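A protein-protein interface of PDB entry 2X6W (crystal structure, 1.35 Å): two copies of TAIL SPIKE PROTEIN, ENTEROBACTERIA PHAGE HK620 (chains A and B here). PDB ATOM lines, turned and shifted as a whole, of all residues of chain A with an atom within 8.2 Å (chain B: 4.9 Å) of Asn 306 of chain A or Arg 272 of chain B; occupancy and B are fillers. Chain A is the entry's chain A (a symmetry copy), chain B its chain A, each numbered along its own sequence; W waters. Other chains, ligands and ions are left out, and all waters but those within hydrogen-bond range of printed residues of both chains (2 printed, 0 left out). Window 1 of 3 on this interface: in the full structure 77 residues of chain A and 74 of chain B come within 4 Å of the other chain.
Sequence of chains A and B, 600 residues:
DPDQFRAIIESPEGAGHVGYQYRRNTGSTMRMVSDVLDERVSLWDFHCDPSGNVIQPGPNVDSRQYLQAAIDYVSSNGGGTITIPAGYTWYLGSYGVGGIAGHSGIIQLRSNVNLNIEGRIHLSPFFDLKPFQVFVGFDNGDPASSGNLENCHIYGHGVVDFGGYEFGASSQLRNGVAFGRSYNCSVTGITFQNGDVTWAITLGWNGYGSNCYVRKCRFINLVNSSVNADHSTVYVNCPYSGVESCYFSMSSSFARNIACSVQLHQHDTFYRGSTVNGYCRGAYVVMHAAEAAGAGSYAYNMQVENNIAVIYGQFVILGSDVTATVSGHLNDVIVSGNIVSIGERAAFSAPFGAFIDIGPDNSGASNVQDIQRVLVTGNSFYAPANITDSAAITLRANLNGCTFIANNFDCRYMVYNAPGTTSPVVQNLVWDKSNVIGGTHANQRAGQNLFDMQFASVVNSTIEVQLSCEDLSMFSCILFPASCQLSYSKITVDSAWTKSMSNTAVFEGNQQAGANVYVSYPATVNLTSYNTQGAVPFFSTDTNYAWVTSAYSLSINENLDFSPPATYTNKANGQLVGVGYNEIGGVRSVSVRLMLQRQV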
ATOM      1  N   GLU A 244      28.643 -27.142  20.253  1.00  0.00           N
ATOM      2  CA  GLU A 244      27.482 -27.170  19.360  1.00  0.00           C
ATOM      3  C   GLU A 244      26.598 -28.379  19.656  1.00  0.00           C
ATOM      4  O   GLU A 244      27.099 -29.487  19.811  1.00  0.00           O
ATOM      5  CB  GLU A 244      28.047 -27.303  17.944  1.00  0.00           C
ATOM      6  CG  GLU A 244      27.236 -27.174  16.734  1.00  0.00           C
ATOM      7  CD  GLU A 244      28.165 -26.813  15.552  1.00  0.00           C
ATOM      8  OE1 GLU A 244      29.176 -27.519  15.271  1.00  0.00           O
ATOM      9  OE2 GLU A 244      27.900 -25.791  14.934  1.00  0.00           O
ATOM     10  N   SER A 245      25.287 -28.161  19.709  1.00  0.00           N
ATOM     11  CA  SER A 245      24.298 -29.254  19.740  1.00  0.00           C
ATOM     12  C   SER A 245      24.529 -30.211  20.888  1.00  0.00           C
ATOM     13  O   SER A 245      24.486 -31.418  20.692  1.00  0.00           O
ATOM     14  CB  SER A 245      24.286 -29.993  18.403  1.00  0.00           C
ATOM     15  OG  SER A 245      23.934 -29.122  17.324  1.00  0.00           O
ATOM     16  N   CYS A 246      24.757 -29.664  22.074  1.00  0.00           N
ATOM     17  CA  CYS A 246      24.932 -30.468  23.273  1.00  0.00           C
ATOM     18  C   CYS A 246      23.731 -30.342  24.191  1.00  0.00           C
ATOM     19  O   CYS A 246      22.838 -29.500  24.015  1.00  0.00           O
ATOM     20  CB  CYS A 246      26.213 -30.035  24.033  1.00  0.00           C
ATOM     21  SG  CYS A 246      27.734 -30.506  23.188  1.00  0.00           S
ATOM     22  N   TYR A 271      29.083 -20.965  21.098  1.00  0.00           N
ATOM     23  CA  TYR A 271      28.221 -21.862  21.857  1.00  0.00           C
ATOM     24  C   TYR A 271      26.858 -21.794  21.184  1.00  0.00           C
ATOM     25  O   TYR A 271      26.195 -20.751  21.230  1.00  0.00           O
ATOM     26  CB  TYR A 271      28.168 -21.420  23.313  1.00  0.00           C
ATOM     27  CG  TYR A 271      27.293 -22.259  24.204  1.00  0.00           C
ATOM     28  CD1 TYR A 271      27.012 -23.604  23.929  1.00  0.00           C
ATOM     29  CD2 TYR A 271      26.735 -21.708  25.354  1.00  0.00           C
ATOM     30  CE1 TYR A 271      26.250 -24.357  24.787  1.00  0.00           C
ATOM     31  CE2 TYR A 271      25.984 -22.480  26.204  1.00  0.00           C
ATOM     32  CZ  TYR A 271      25.735 -23.794  25.926  1.00  0.00           C
ATOM     33  OH  TYR A 271      24.972 -24.550  26.805  1.00  0.00           O
ATOM     34  N   ARG A 272      26.453 -22.891  20.528  1.00  0.00           N
ATOM     35  CA  ARG A 272      25.262 -22.852  19.713  1.00  0.00           C
ATOM     36  C   ARG A 272      24.417 -24.103  19.836  1.00  0.00           C
ATOM     37  O   ARG A 272      24.911 -25.215  20.080  1.00  0.00           O
ATOM     38  CB  ARG A 272      25.666 -22.791  18.226  1.00  0.00           C
ATOM     39  CG  ARG A 272      26.494 -21.583  17.785  1.00  0.00           C
ATOM     40  CD  ARG A 272      26.448 -21.389  16.270  1.00  0.00           C
ATOM     41  NE  ARG A 272      27.146 -22.472  15.572  1.00  0.00           N
ATOM     42  CZ  ARG A 272      28.362 -22.396  15.015  1.00  0.00           C
ATOM     43  NH1 ARG A 272      29.077 -21.278  15.033  1.00  0.00           N
ATOM     44  NH2 ARG A 272      28.866 -23.465  14.409  1.00  0.00           N
ATOM     45  N   GLY A 273      23.124 -23.915  19.639  1.00  0.00           N
ATOM     46  CA  GLY A 273      22.246 -25.048  19.405  1.00  0.00           C
ATOM     47  C   GLY A 273      22.127 -26.063  20.513  1.00  0.00           C
ATOM     48  O   GLY A 273      21.837 -27.229  20.250  1.00  0.00           O
ATOM     49  N   SER A 274      22.331 -25.640  21.755  1.00  0.00           N
ATOM     50  CA  SER A 274      22.399 -26.533  22.872  1.00  0.00           C
ATOM     51  C   SER A 274      21.224 -26.277  23.808  1.00  0.00           C
ATOM     52  O   SER A 274      20.583 -25.237  23.752  1.00  0.00           O
ATOM     53  CB  SER A 274      23.725 -26.349  23.584  1.00  0.00           C
ATOM     54  OG  SER A 274      24.810 -26.706  22.730  1.00  0.00           O
ATOM     55  N   THR A 275      20.945 -27.267  24.647  1.00  0.00           N
ATOM     56  CA  THR A 275      19.855 -27.219  25.612  1.00  0.00           C
ATOM     57  C   THR A 275      20.439 -27.422  27.008  1.00  0.00           C
ATOM     58  O   THR A 275      21.215 -28.349  27.232  1.00  0.00           O
ATOM     59  CB  THR A 275      18.786 -28.303  25.332  1.00  0.00           C
ATOM     60  OG1 THR A 275      18.172 -28.052  24.057  1.00  0.00           O
ATOM     61  CG2 THR A 275      17.688 -28.332  26.426  1.00  0.00           C
ATOM     62  N   GLN A 303      30.302 -15.851  20.051  1.00  0.00           N
ATOM     63  CA  GLN A 303      28.955 -16.121  19.559  1.00  0.00           C
ATOM     64  C   GLN A 303      28.184 -17.070  20.482  1.00  0.00           C
ATOM     65  O   GLN A 303      28.653 -18.154  20.786  1.00  0.00           O
ATOM     66  CB  GLN A 303      29.089 -16.711  18.171  1.00  0.00           C
ATOM     67  CG  GLN A 303      27.796 -16.991  17.474  1.00  0.00           C
ATOM     68  CD  GLN A 303      28.030 -17.807  16.216  1.00  0.00           C
ATOM     69  OE1 GLN A 303      28.433 -18.955  16.298  1.00  0.00           O
ATOM     70  NE2 GLN A 303      27.768 -17.218  15.055  1.00  0.00           N
ATOM     71  N   VAL A 304      27.026 -16.614  20.969  1.00  0.00           N
ATOM     72  CA  VAL A 304      26.140 -17.445  21.775  1.00  0.00           C
ATOM     73  C   VAL A 304      24.783 -17.404  21.075  1.00  0.00           C
ATOM     74  O   VAL A 304      24.079 -16.383  21.128  1.00  0.00           O
ATOM     75  CB  VAL A 304      26.009 -16.959  23.226  1.00  0.00           C
ATOM     76  CG1 VAL A 304      25.025 -17.830  23.997  1.00  0.00           C
ATOM     77  CG2 VAL A 304      27.376 -16.965  23.933  1.00  0.00           C
ATOM     78  N   GLU A 305      24.420 -18.499  20.394  1.00  0.00           N
ATOM     79  CA  GLU A 305      23.261 -18.467  19.491  1.00  0.00           C
ATOM     80  C   GLU A 305      22.411 -19.720  19.545  1.00  0.00           C
ATOM     81  O   GLU A 305      22.902 -20.849  19.614  1.00  0.00           O
ATOM     82  CB  GLU A 305      23.703 -18.241  18.031  1.00  0.00           C
ATOM     83  CG  GLU A 305      24.147 -16.816  17.778  1.00  0.00           C
ATOM     84  CD  GLU A 305      24.594 -16.510  16.347  1.00  0.00           C
ATOM     85  OE1 GLU A 305      25.001 -17.444  15.630  1.00  0.00           O
ATOM     86  OE2 GLU A 305      24.578 -15.315  15.975  1.00  0.00           O
ATOM     87  N   ASN A 306      21.108 -19.495  19.479  1.00  0.00           N
ATOM     88  CA  ASN A 306      20.145 -20.552  19.226  1.00  0.00           C
ATOM     89  C   ASN A 306      20.155 -21.670  20.280  1.00  0.00           C
ATOM     90  O   ASN A 306      19.926 -22.826  19.977  1.00  0.00           O
ATOM     91  CB  ASN A 306      20.345 -21.181  17.824  1.00  0.00           C
ATOM     92  CG  ASN A 306      20.044 -20.224  16.678  1.00  0.00           C
ATOM     93  OD1 ASN A 306      19.784 -19.047  16.877  1.00  0.00           O
ATOM     94  ND2 ASN A 306      20.097 -20.749  15.452  1.00  0.00           N
ATOM     95  N   ASN A 307      20.394 -21.286  21.519  1.00  0.00           N
ATOM     96  CA  ASN A 307      20.340 -22.194  22.651  1.00  0.00           C
ATOM     97  C   ASN A 307      18.973 -22.115  23.354  1.00  0.00           C
ATOM     98  O   ASN A 307      18.237 -21.143  23.223  1.00  0.00           O
ATOM     99  CB  ASN A 307      21.447 -21.900  23.639  1.00  0.00           C
ATOM    100  CG  ASN A 307      22.817 -21.990  22.997  1.00  0.00           C
ATOM    101  OD1 ASN A 307      23.250 -23.077  22.600  1.00  0.00           O
ATOM    102  ND2 ASN A 307      23.521 -20.855  22.904  1.00  0.00           N
ATOM    103  N   ILE A 308      18.662 -23.163  24.102  1.00  0.00           N
ATOM    104  CA  ILE A 308      17.439 -23.299  24.890  1.00  0.00           C
ATOM    105  C   ILE A 308      17.902 -23.521  26.323  1.00  0.00           C
ATOM    106  O   ILE A 308      18.715 -24.403  26.565  1.00  0.00           O
ATOM    107  CB  ILE A 308      16.638 -24.537  24.415  1.00  0.00           C
ATOM    108  CG1 ILE A 308      16.266 -24.411  22.922  1.00  0.00           C
ATOM    109  CG2 ILE A 308      15.415 -24.733  25.313  1.00  0.00           C
ATOM    110  CD1 ILE A 308      15.722 -25.725  22.291  1.00  0.00           C
ATOM    111  N   ALA A 309      17.402 -22.738  27.271  1.00  0.00           N
ATOM    112  CA  ALA A 309      17.883 -22.868  28.648  1.00  0.00           C
ATOM    113  C   ALA A 309      16.805 -22.611  29.696  1.00  0.00           C
ATOM    114  O   ALA A 309      15.937 -21.729  29.538  1.00  0.00           O
ATOM    115  CB  ALA A 309      19.096 -21.955  28.881  1.00  0.00           C
ATOM    116  N   PHE A 315      22.025 -15.911  32.306  1.00  0.00           N
ATOM    117  CA  PHE A 315      22.258 -16.639  31.059  1.00  0.00           C
ATOM    118  C   PHE A 315      23.647 -16.410  30.464  1.00  0.00           C
ATOM    119  O   PHE A 315      24.419 -17.364  30.328  1.00  0.00           O
ATOM    120  CB  PHE A 315      21.170 -16.344  30.039  1.00  0.00           C
ATOM    121  CG  PHE A 315      21.357 -17.084  28.749  1.00  0.00           C
ATOM    122  CD1 PHE A 315      21.439 -18.471  28.730  1.00  0.00           C
ATOM    123  CD2 PHE A 315      21.542 -16.401  27.560  1.00  0.00           C
ATOM    124  CE1 PHE A 315      21.677 -19.167  27.559  1.00  0.00           C
ATOM    125  CE2 PHE A 315      21.736 -17.097  26.363  1.00  0.00           C
ATOM    126  CZ  PHE A 315      21.811 -18.474  26.375  1.00  0.00           C
ATOM    127  N   ILE A 334      28.129 -11.499  19.842  1.00  0.00           N
ATOM    128  CA  ILE A 334      26.722 -11.597  19.406  1.00  0.00           C
ATOM    129  C   ILE A 334      26.008 -12.672  20.220  1.00  0.00           C
ATOM    130  O   ILE A 334      26.510 -13.782  20.369  1.00  0.00           O
ATOM    131  CB  ILE A 334      26.596 -11.821  17.873  1.00  0.00           C
ATOM    132  CG1 ILE A 334      25.140 -11.632  17.405  1.00  0.00           C
ATOM    133  CG2 ILE A 334      27.213 -13.167  17.429  1.00  0.00           C
ATOM    134  CD1 ILE A 334      24.963 -11.497  15.912  1.00  0.00           C
ATOM    135  N   VAL A 335      24.857 -12.286  20.772  1.00  0.00           N
ATOM    136  CA  VAL A 335      23.981 -13.171  21.546  1.00  0.00           C
ATOM    137  C   VAL A 335      22.625 -13.109  20.854  1.00  0.00           C
ATOM    138  O   VAL A 335      21.958 -12.085  20.904  1.00  0.00           O
ATOM    139  CB  VAL A 335      23.873 -12.742  23.032  1.00  0.00           C
ATOM    140  CG1 VAL A 335      22.928 -13.672  23.789  1.00  0.00           C
ATOM    141  CG2 VAL A 335      25.262 -12.663  23.681  1.00  0.00           C
ATOM    142  N   SER A 336      22.243 -14.184  20.175  1.00  0.00           N
ATOM    143  CA  SER A 336      21.059 -14.147  19.326  1.00  0.00           C
ATOM    144  C   SER A 336      20.310 -15.465  19.275  1.00  0.00           C
ATOM    145  O   SER A 336      20.907 -16.528  19.282  1.00  0.00           O
ATOM    146  CB  SER A 336      21.442 -13.737  17.904  1.00  0.00           C
ATOM    147  OG  SER A 336      22.220 -14.732  17.273  1.00  0.00           O
ATOM    148  N   GLY A 337      18.978 -15.395  19.161  1.00  0.00           N
ATOM    149  CA  GLY A 337      18.168 -16.559  18.894  1.00  0.00           C
ATOM    150  C   GLY A 337      17.978 -17.486  20.065  1.00  0.00           C
ATOM    151  O   GLY A 337      17.470 -18.580  19.887  1.00  0.00           O
ATOM    152  N   ASN A 338      18.371 -17.064  21.256  1.00  0.00           N
ATOM    153  CA  ASN A 338      18.268 -17.924  22.449  1.00  0.00           C
ATOM    154  C   ASN A 338      16.894 -17.779  23.095  1.00  0.00           C
ATOM    155  O   ASN A 338      16.313 -16.680  23.092  1.00  0.00           O
ATOM    156  CB  ASN A 338      19.340 -17.564  23.471  1.00  0.00           C
ATOM    157  CG  ASN A 338      20.730 -17.663  22.888  1.00  0.00           C
ATOM    158  OD1 ASN A 338      21.272 -18.756  22.763  1.00  0.00           O
ATOM    159  ND2 ASN A 338      21.338 -16.504  22.579  1.00  0.00           N
ATOM    160  N   ILE A 339      16.375 -18.882  23.639  1.00  0.00           N
ATOM    161  CA  ILE A 339      15.138 -18.863  24.406  1.00  0.00           C
ATOM    162  C   ILE A 339      15.461 -19.360  25.804  1.00  0.00           C
ATOM    163  O   ILE A 339      15.948 -20.483  25.984  1.00  0.00           O
ATOM    164  CB  ILE A 339      13.982 -19.647  23.698  1.00  0.00           C
ATOM    165  CG1 ILE A 339      12.740 -19.590  24.561  1.00  0.00           C
ATOM    166  CG2 ILE A 339      14.325 -21.092  23.345  1.00  0.00           C
ATOM    167  CD1 ILE A 339      11.442 -19.785  23.827  1.00  0.00           C
ATOM    168  N   VAL A 340      15.234 -18.490  26.782  1.00  0.00           N
ATOM    169  CA  VAL A 340      15.771 -18.695  28.134  1.00  0.00           C
ATOM    170  C   VAL A 340      14.716 -18.312  29.149  1.00  0.00           C
ATOM    171  O   VAL A 340      14.019 -17.320  28.998  1.00  0.00           O
ATOM    172  CB  VAL A 340      17.055 -17.856  28.397  1.00  0.00           C
ATOM    173  CG1 VAL A 340      17.571 -18.105  29.799  1.00  0.00           C
ATOM    174  CG2 VAL A 340      18.156 -18.187  27.334  1.00  0.00           C
ATOM    175  N   THR A 377      20.354  -9.665  20.295  1.00  0.00           N
ATOM    176  CA  THR A 377      19.250  -9.498  19.374  1.00  0.00           C
ATOM    177  C   THR A 377      18.474 -10.789  19.177  1.00  0.00           C
ATOM    178  O   THR A 377      19.032 -11.865  19.099  1.00  0.00           O
ATOM    179  CB  THR A 377      19.725  -8.911  18.018  1.00  0.00           C
ATOM    180  OG1 THR A 377      18.600  -8.585  17.216  1.00  0.00           O
ATOM    181  CG2 THR A 377      20.626  -9.832  17.267  1.00  0.00           C
ATOM    182  N   GLY A 378      17.159 -10.650  19.100  1.00  0.00           N
ATOM    183  CA  GLY A 378      16.307 -11.760  18.706  1.00  0.00           C
ATOM    184  C   GLY A 378      16.247 -12.889  19.698  1.00  0.00           C
ATOM    185  O   GLY A 378      16.149 -14.046  19.299  1.00  0.00           O
ATOM    186  N   ASN A 379      16.345 -12.550  20.980  1.00  0.00           N
ATOM    187  CA  ASN A 379      16.233 -13.510  22.080  1.00  0.00           C
ATOM    188  C   ASN A 379      14.937 -13.332  22.813  1.00  0.00           C
ATOM    189  O   ASN A 379      14.328 -12.272  22.772  1.00  0.00           O
ATOM    190  CB  ASN A 379      17.353 -13.303  23.119  1.00  0.00           C
ATOM    191  CG  ASN A 379      18.748 -13.352  22.500  1.00  0.00           C
ATOM    192  OD1 ASN A 379      19.278 -14.432  22.242  1.00  0.00           O
ATOM    193  ND2 ASN A 379      19.363 -12.185  22.319  1.00  0.00           N
ATOM    194  N   VAL B 243      14.987 -32.216  15.685  1.00  0.00           N
ATOM    195  CA  VAL B 243      15.319 -32.480  14.282  1.00  0.00           C
ATOM    196  C   VAL B 243      16.263 -31.376  13.807  1.00  0.00           C
ATOM    197  O   VAL B 243      15.947 -30.203  13.980  1.00  0.00           O
ATOM    198  CB  VAL B 243      14.034 -32.466  13.421  1.00  0.00           C
ATOM    199  CG1 VAL B 243      14.374 -32.612  11.934  1.00  0.00           C
ATOM    200  CG2 VAL B 243      13.054 -33.534  13.932  1.00  0.00           C
ATOM    201  N   GLU B 244      17.394 -31.756  13.194  1.00  0.00           N
ATOM    202  CA  GLU B 244      18.425 -30.811  12.763  1.00  0.00           C
ATOM    203  C   GLU B 244      19.000 -31.215  11.408  1.00  0.00           C
ATOM    204  O   GLU B 244      19.310 -32.381  11.192  1.00  0.00           O
ATOM    205  CB  GLU B 244      19.534 -30.893  13.815  1.00  0.00           C
ATOM    206  CG  GLU B 244      20.666 -29.970  13.872  1.00  0.00           C
ATOM    207  CD  GLU B 244      21.244 -29.982  15.306  1.00  0.00           C
ATOM    208  OE1 GLU B 244      21.591 -31.062  15.865  1.00  0.00           O
ATOM    209  OE2 GLU B 244      21.305 -28.906  15.885  1.00  0.00           O
ATOM    210  N   SER B 245      19.159 -30.243  10.513  1.00  0.00           N
ATOM    211  CA  SER B 245      19.920 -30.426   9.264  1.00  0.00           C
ATOM    212  C   SER B 245      19.393 -31.572   8.429  1.00  0.00           C
ATOM    213  O   SER B 245      20.175 -32.375   7.937  1.00  0.00           O
ATOM    214  CB  SER B 245      21.405 -30.608   9.573  1.00  0.00           C
ATOM    215  OG  SER B 245      21.946 -29.467  10.246  1.00  0.00           O
ATOM    216  N   CYS B 246      18.079 -31.627   8.266  1.00  0.00           N
ATOM    217  CA  CYS B 246      17.447 -32.639   7.435  1.00  0.00           C
ATOM    218  C   CYS B 246      16.908 -32.031   6.154  1.00  0.00           C
ATOM    219  O   CYS B 246      16.843 -30.806   5.970  1.00  0.00           O
ATOM    220  CB  CYS B 246      16.292 -33.330   8.207  1.00  0.00           C
ATOM    221  SG  CYS B 246      16.867 -34.411   9.529  1.00  0.00           S
ATOM    222  N   PHE B 270      13.065 -28.993  19.343  1.00  0.00           N
ATOM    223  CA  PHE B 270      13.556 -28.097  18.315  1.00  0.00           C
ATOM    224  C   PHE B 270      13.510 -28.669  16.902  1.00  0.00           C
ATOM    225  O   PHE B 270      13.542 -29.881  16.689  1.00  0.00           O
ATOM    226  CB  PHE B 270      14.980 -27.648  18.623  1.00  0.00           C
ATOM    227  CG  PHE B 270      15.996 -28.763  18.689  1.00  0.00           C
ATOM    228  CD1 PHE B 270      16.630 -29.216  17.547  1.00  0.00           C
ATOM    229  CD2 PHE B 270      16.317 -29.359  19.892  1.00  0.00           C
ATOM    230  CE1 PHE B 270      17.564 -30.240  17.596  1.00  0.00           C
ATOM    231  CE2 PHE B 270      17.254 -30.378  19.948  1.00  0.00           C
ATOM    232  CZ  PHE B 270      17.877 -30.820  18.806  1.00  0.00           C
ATOM    233  N   TYR B 271      13.474 -27.742  15.950  1.00  0.00           N
ATOM    234  CA  TYR B 271      13.502 -28.053  14.526  1.00  0.00           C
ATOM    235  C   TYR B 271      14.351 -26.968  13.881  1.00  0.00           C
ATOM    236  O   TYR B 271      13.946 -25.800  13.849  1.00  0.00           O
ATOM    237  CB  TYR B 271      12.083 -28.078  13.975  1.00  0.00           C
ATOM    238  CG  TYR B 271      11.974 -28.374  12.503  1.00  0.00           C
ATOM    239  CD1 TYR B 271      12.948 -29.107  11.811  1.00  0.00           C
ATOM    240  CD2 TYR B 271      10.876 -27.920  11.779  1.00  0.00           C
ATOM    241  CE1 TYR B 271      12.796 -29.402  10.480  1.00  0.00           C
ATOM    242  CE2 TYR B 271      10.738 -28.234  10.450  1.00  0.00           C
ATOM    243  CZ  TYR B 271      11.690 -28.964   9.797  1.00  0.00           C
ATOM    244  OH  TYR B 271      11.524 -29.266   8.454  1.00  0.00           O
ATOM    245  N   ARG B 272      15.546 -27.341  13.400  1.00  0.00           N
ATOM    246  CA  ARG B 272      16.486 -26.350  12.939  1.00  0.00           C
ATOM    247  C   ARG B 272      17.216 -26.763  11.678  1.00  0.00           C
ATOM    248  O   ARG B 272      17.457 -27.951  11.411  1.00  0.00           O
ATOM    249  CB  ARG B 272      17.594 -26.170  13.997  1.00  0.00           C
ATOM    250  CG  ARG B 272      17.154 -25.693  15.382  1.00  0.00           C
ATOM    251  CD  ARG B 272      18.325 -25.125  16.183  1.00  0.00           C
ATOM    252  NE  ARG B 272      19.283 -26.173  16.543  1.00  0.00           N
ATOM    253  CZ  ARG B 272      19.417 -26.739  17.751  1.00  0.00           C
ATOM    254  NH1 ARG B 272      18.668 -26.377  18.785  1.00  0.00           N
ATOM    255  NH2 ARG B 272      20.338 -27.678  17.929  1.00  0.00           N
ATOM    256  N   GLY B 273      17.594 -25.759  10.907  1.00  0.00           N
ATOM    257  CA  GLY B 273      18.569 -25.971   9.851  1.00  0.00           C
ATOM    258  C   GLY B 273      18.188 -26.929   8.750  1.00  0.00           C
ATOM    259  O   GLY B 273      19.064 -27.529   8.128  1.00  0.00           O
ATOM    260  N   SER B 274      16.895 -27.074   8.485  1.00  0.00           N
ATOM    261  CA  SER B 274      16.401 -28.062   7.573  1.00  0.00           C
ATOM    262  C   SER B 274      15.776 -27.380   6.363  1.00  0.00           C
ATOM    263  O   SER B 274      15.451 -26.202   6.396  1.00  0.00           O
ATOM    264  CB  SER B 274      15.402 -28.950   8.288  1.00  0.00           C
ATOM    265  OG  SER B 274      16.031 -29.671   9.345  1.00  0.00           O
ATOM    266  N   GLN B 303      11.476 -24.499  19.722  1.00  0.00           N
ATOM    267  CA  GLN B 303      12.342 -23.718  18.844  1.00  0.00           C
ATOM    268  C   GLN B 303      12.237 -24.167  17.383  1.00  0.00           C
ATOM    269  O   GLN B 303      12.420 -25.335  17.081  1.00  0.00           O
ATOM    270  CB  GLN B 303      13.760 -23.870  19.354  1.00  0.00           C
ATOM    271  CG  GLN B 303      14.788 -23.077  18.613  1.00  0.00           C
ATOM    272  CD  GLN B 303      16.187 -23.490  19.029  1.00  0.00           C
ATOM    273  OE1 GLN B 303      16.602 -24.605  18.757  1.00  0.00           O
ATOM    274  NE2 GLN B 303      16.917 -22.590  19.678  1.00  0.00           N
ATOM    275  N   GLU B 305      13.929 -22.816  13.988  1.00  0.00           N
ATOM    276  CA  GLU B 305      14.940 -21.826  13.590  1.00  0.00           C
ATOM    277  C   GLU B 305      15.728 -22.220  12.359  1.00  0.00           C
ATOM    278  O   GLU B 305      16.123 -23.371  12.168  1.00  0.00           O
ATOM    279  CB  GLU B 305      15.933 -21.556  14.740  1.00  0.00           C
ATOM    280  CG  GLU B 305      15.319 -20.728  15.848  1.00  0.00           C
ATOM    281  CD  GLU B 305      16.245 -20.411  17.024  1.00  0.00           C
ATOM    282  OE1 GLU B 305      17.214 -21.162  17.247  1.00  0.00           O
ATOM    283  OE2 GLU B 305      15.956 -19.431  17.746  1.00  0.00           O
ATOM    284  N   ASN B 306      15.981 -21.216  11.533  1.00  0.00           N
ATOM    285  CA  ASN B 306      16.953 -21.315  10.459  1.00  0.00           C
ATOM    286  C   ASN B 306      16.640 -22.415   9.432  1.00  0.00           C
ATOM    287  O   ASN B 306      17.528 -23.035   8.880  1.00  0.00           O
ATOM    288  CB  ASN B 306      18.387 -21.533  11.007  1.00  0.00           C
ATOM    289  CG  ASN B 306      18.928 -20.344  11.789  1.00  0.00           C
ATOM    290  OD1 ASN B 306      18.232 -19.372  12.041  1.00  0.00           O
ATOM    291  ND2 ASN B 306      20.197 -20.439  12.189  1.00  0.00           N
ATOM    292  N   ASN B 307      15.360 -22.609   9.177  1.00  0.00           N
ATOM    293  CA  ASN B 307      14.891 -23.535   8.161  1.00  0.00           C
ATOM    294  C   ASN B 307      14.594 -22.801   6.842  1.00  0.00           C
ATOM    295  O   ASN B 307      14.389 -21.592   6.810  1.00  0.00           O
ATOM    296  CB  ASN B 307      13.658 -24.278   8.628  1.00  0.00           C
ATOM    297  CG  ASN B 307      13.909 -25.039   9.915  1.00  0.00           C
ATOM    298  OD1 ASN B 307      14.684 -26.002   9.929  1.00  0.00           O
ATOM    299  ND2 ASN B 307      13.247 -24.629  11.003  1.00  0.00           N
HETATM  300  O   HOH W   1      19.525 -28.231  21.594  1.00  0.00           O
HETATM  301  O   HOH W   2      17.665 -17.997  14.643  1.00  0.00           O
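Asn 306 of chain A touches Arg 272 of chain B, but with the chains exchanged Arg 272 of chain A does not touch Asn 306 of chain B (7.5 Å).
Of the 9 pairs that touch across the chains among the printed residues, 1 has its exchanged pair printed and touching as well.
Water W1 lies within hydrogen-bond range of the side-chain hydroxyl of Thr 275 of chain A (2.8 Å), the backbone carbonyl oxygen of Gly 273 of chain A (2.9 Å) and the guanidinium group of Arg 272 of chain B (3.5 Å).
O of Glu 305 of chain A is in hydrogen-bond range of N of Gly 273 of chain A, at 3.1 Å.
The backbone NH (N) of Gly 337 of chain A lies within hydrogen-bond range of the side-chain amide oxygen (OD1) of Asn 379 of chain A, 3.2 Å away.
The side-chain carboxylate (OE2) of Glu 244 of chain B is in hydrogen-bond range of the side-chain hydroxyl (OG) of Ser 245 of chain A, at 3.0 Å.
The guanidinium group of Arg 272 of chain B lies within hydrogen-bond range of the backbone carbonyl oxygen of Gly 273 of chain A, 2.8 Å away.
The backbone carbonyl oxygen (O) of Asn 306 of chain A is in hydrogen-bond range of the side-chain amide nitrogen (NE2) of Gln 303 of chain B.
The side-chain carboxylate (OE1) of Glu 305 of chain B sits close to the side-chain amide oxygen (OD1) of Asn 306 of chain A (3.3 Å).
ND2 of Asn 306 of chain B lies close to ND2 of Asn 306 of chain A, at 3.3 Å.
The side-chain carboxylate (OE2) of Glu 305 of chain B sits close to the backbone carbonyl oxygen (O) of Gly 337 of chain A, 2.8 Å away.
Among the printed residues, merely in contact across the chains: Ser 245 of chain A with Arg 272 of chain B, Asn 306 of chain A with Arg 272 of chain B and Ile 308 of chain A with Gln 303 of chain B.
Printed residues of chain A within 4 Å of Glu 244 of chain B: Ser 245.
Of the printed residues of chain A, Gln 303 of chain B touches Asn 306 (3.0 Å) and Ile 308 (3.8 Å).
Printed residues of chain A within 4 Å of Glu 305 of chain B: Asn 306 and Gly 337.
The nearest printed residue of chain B that does not touch Asn 306 of chain A is Phe 270 of chain B (7.0 Å).
The nearest printed residue of chain A that does not touch Arg 272 of chain B is Ile 308 of chain A (4.6 Å).
Of the 13 printed residues of chain B, 5 touch a printed residue of chain A.
Hydrophobic or aromatic side chains of chain A within 4 Å of the printed part of chain B: Ile 308.
Among the printed residues, no Asp or Glu carboxylate lies within 4 Å of a Lys or Arg side-chain nitrogen of the other chain.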
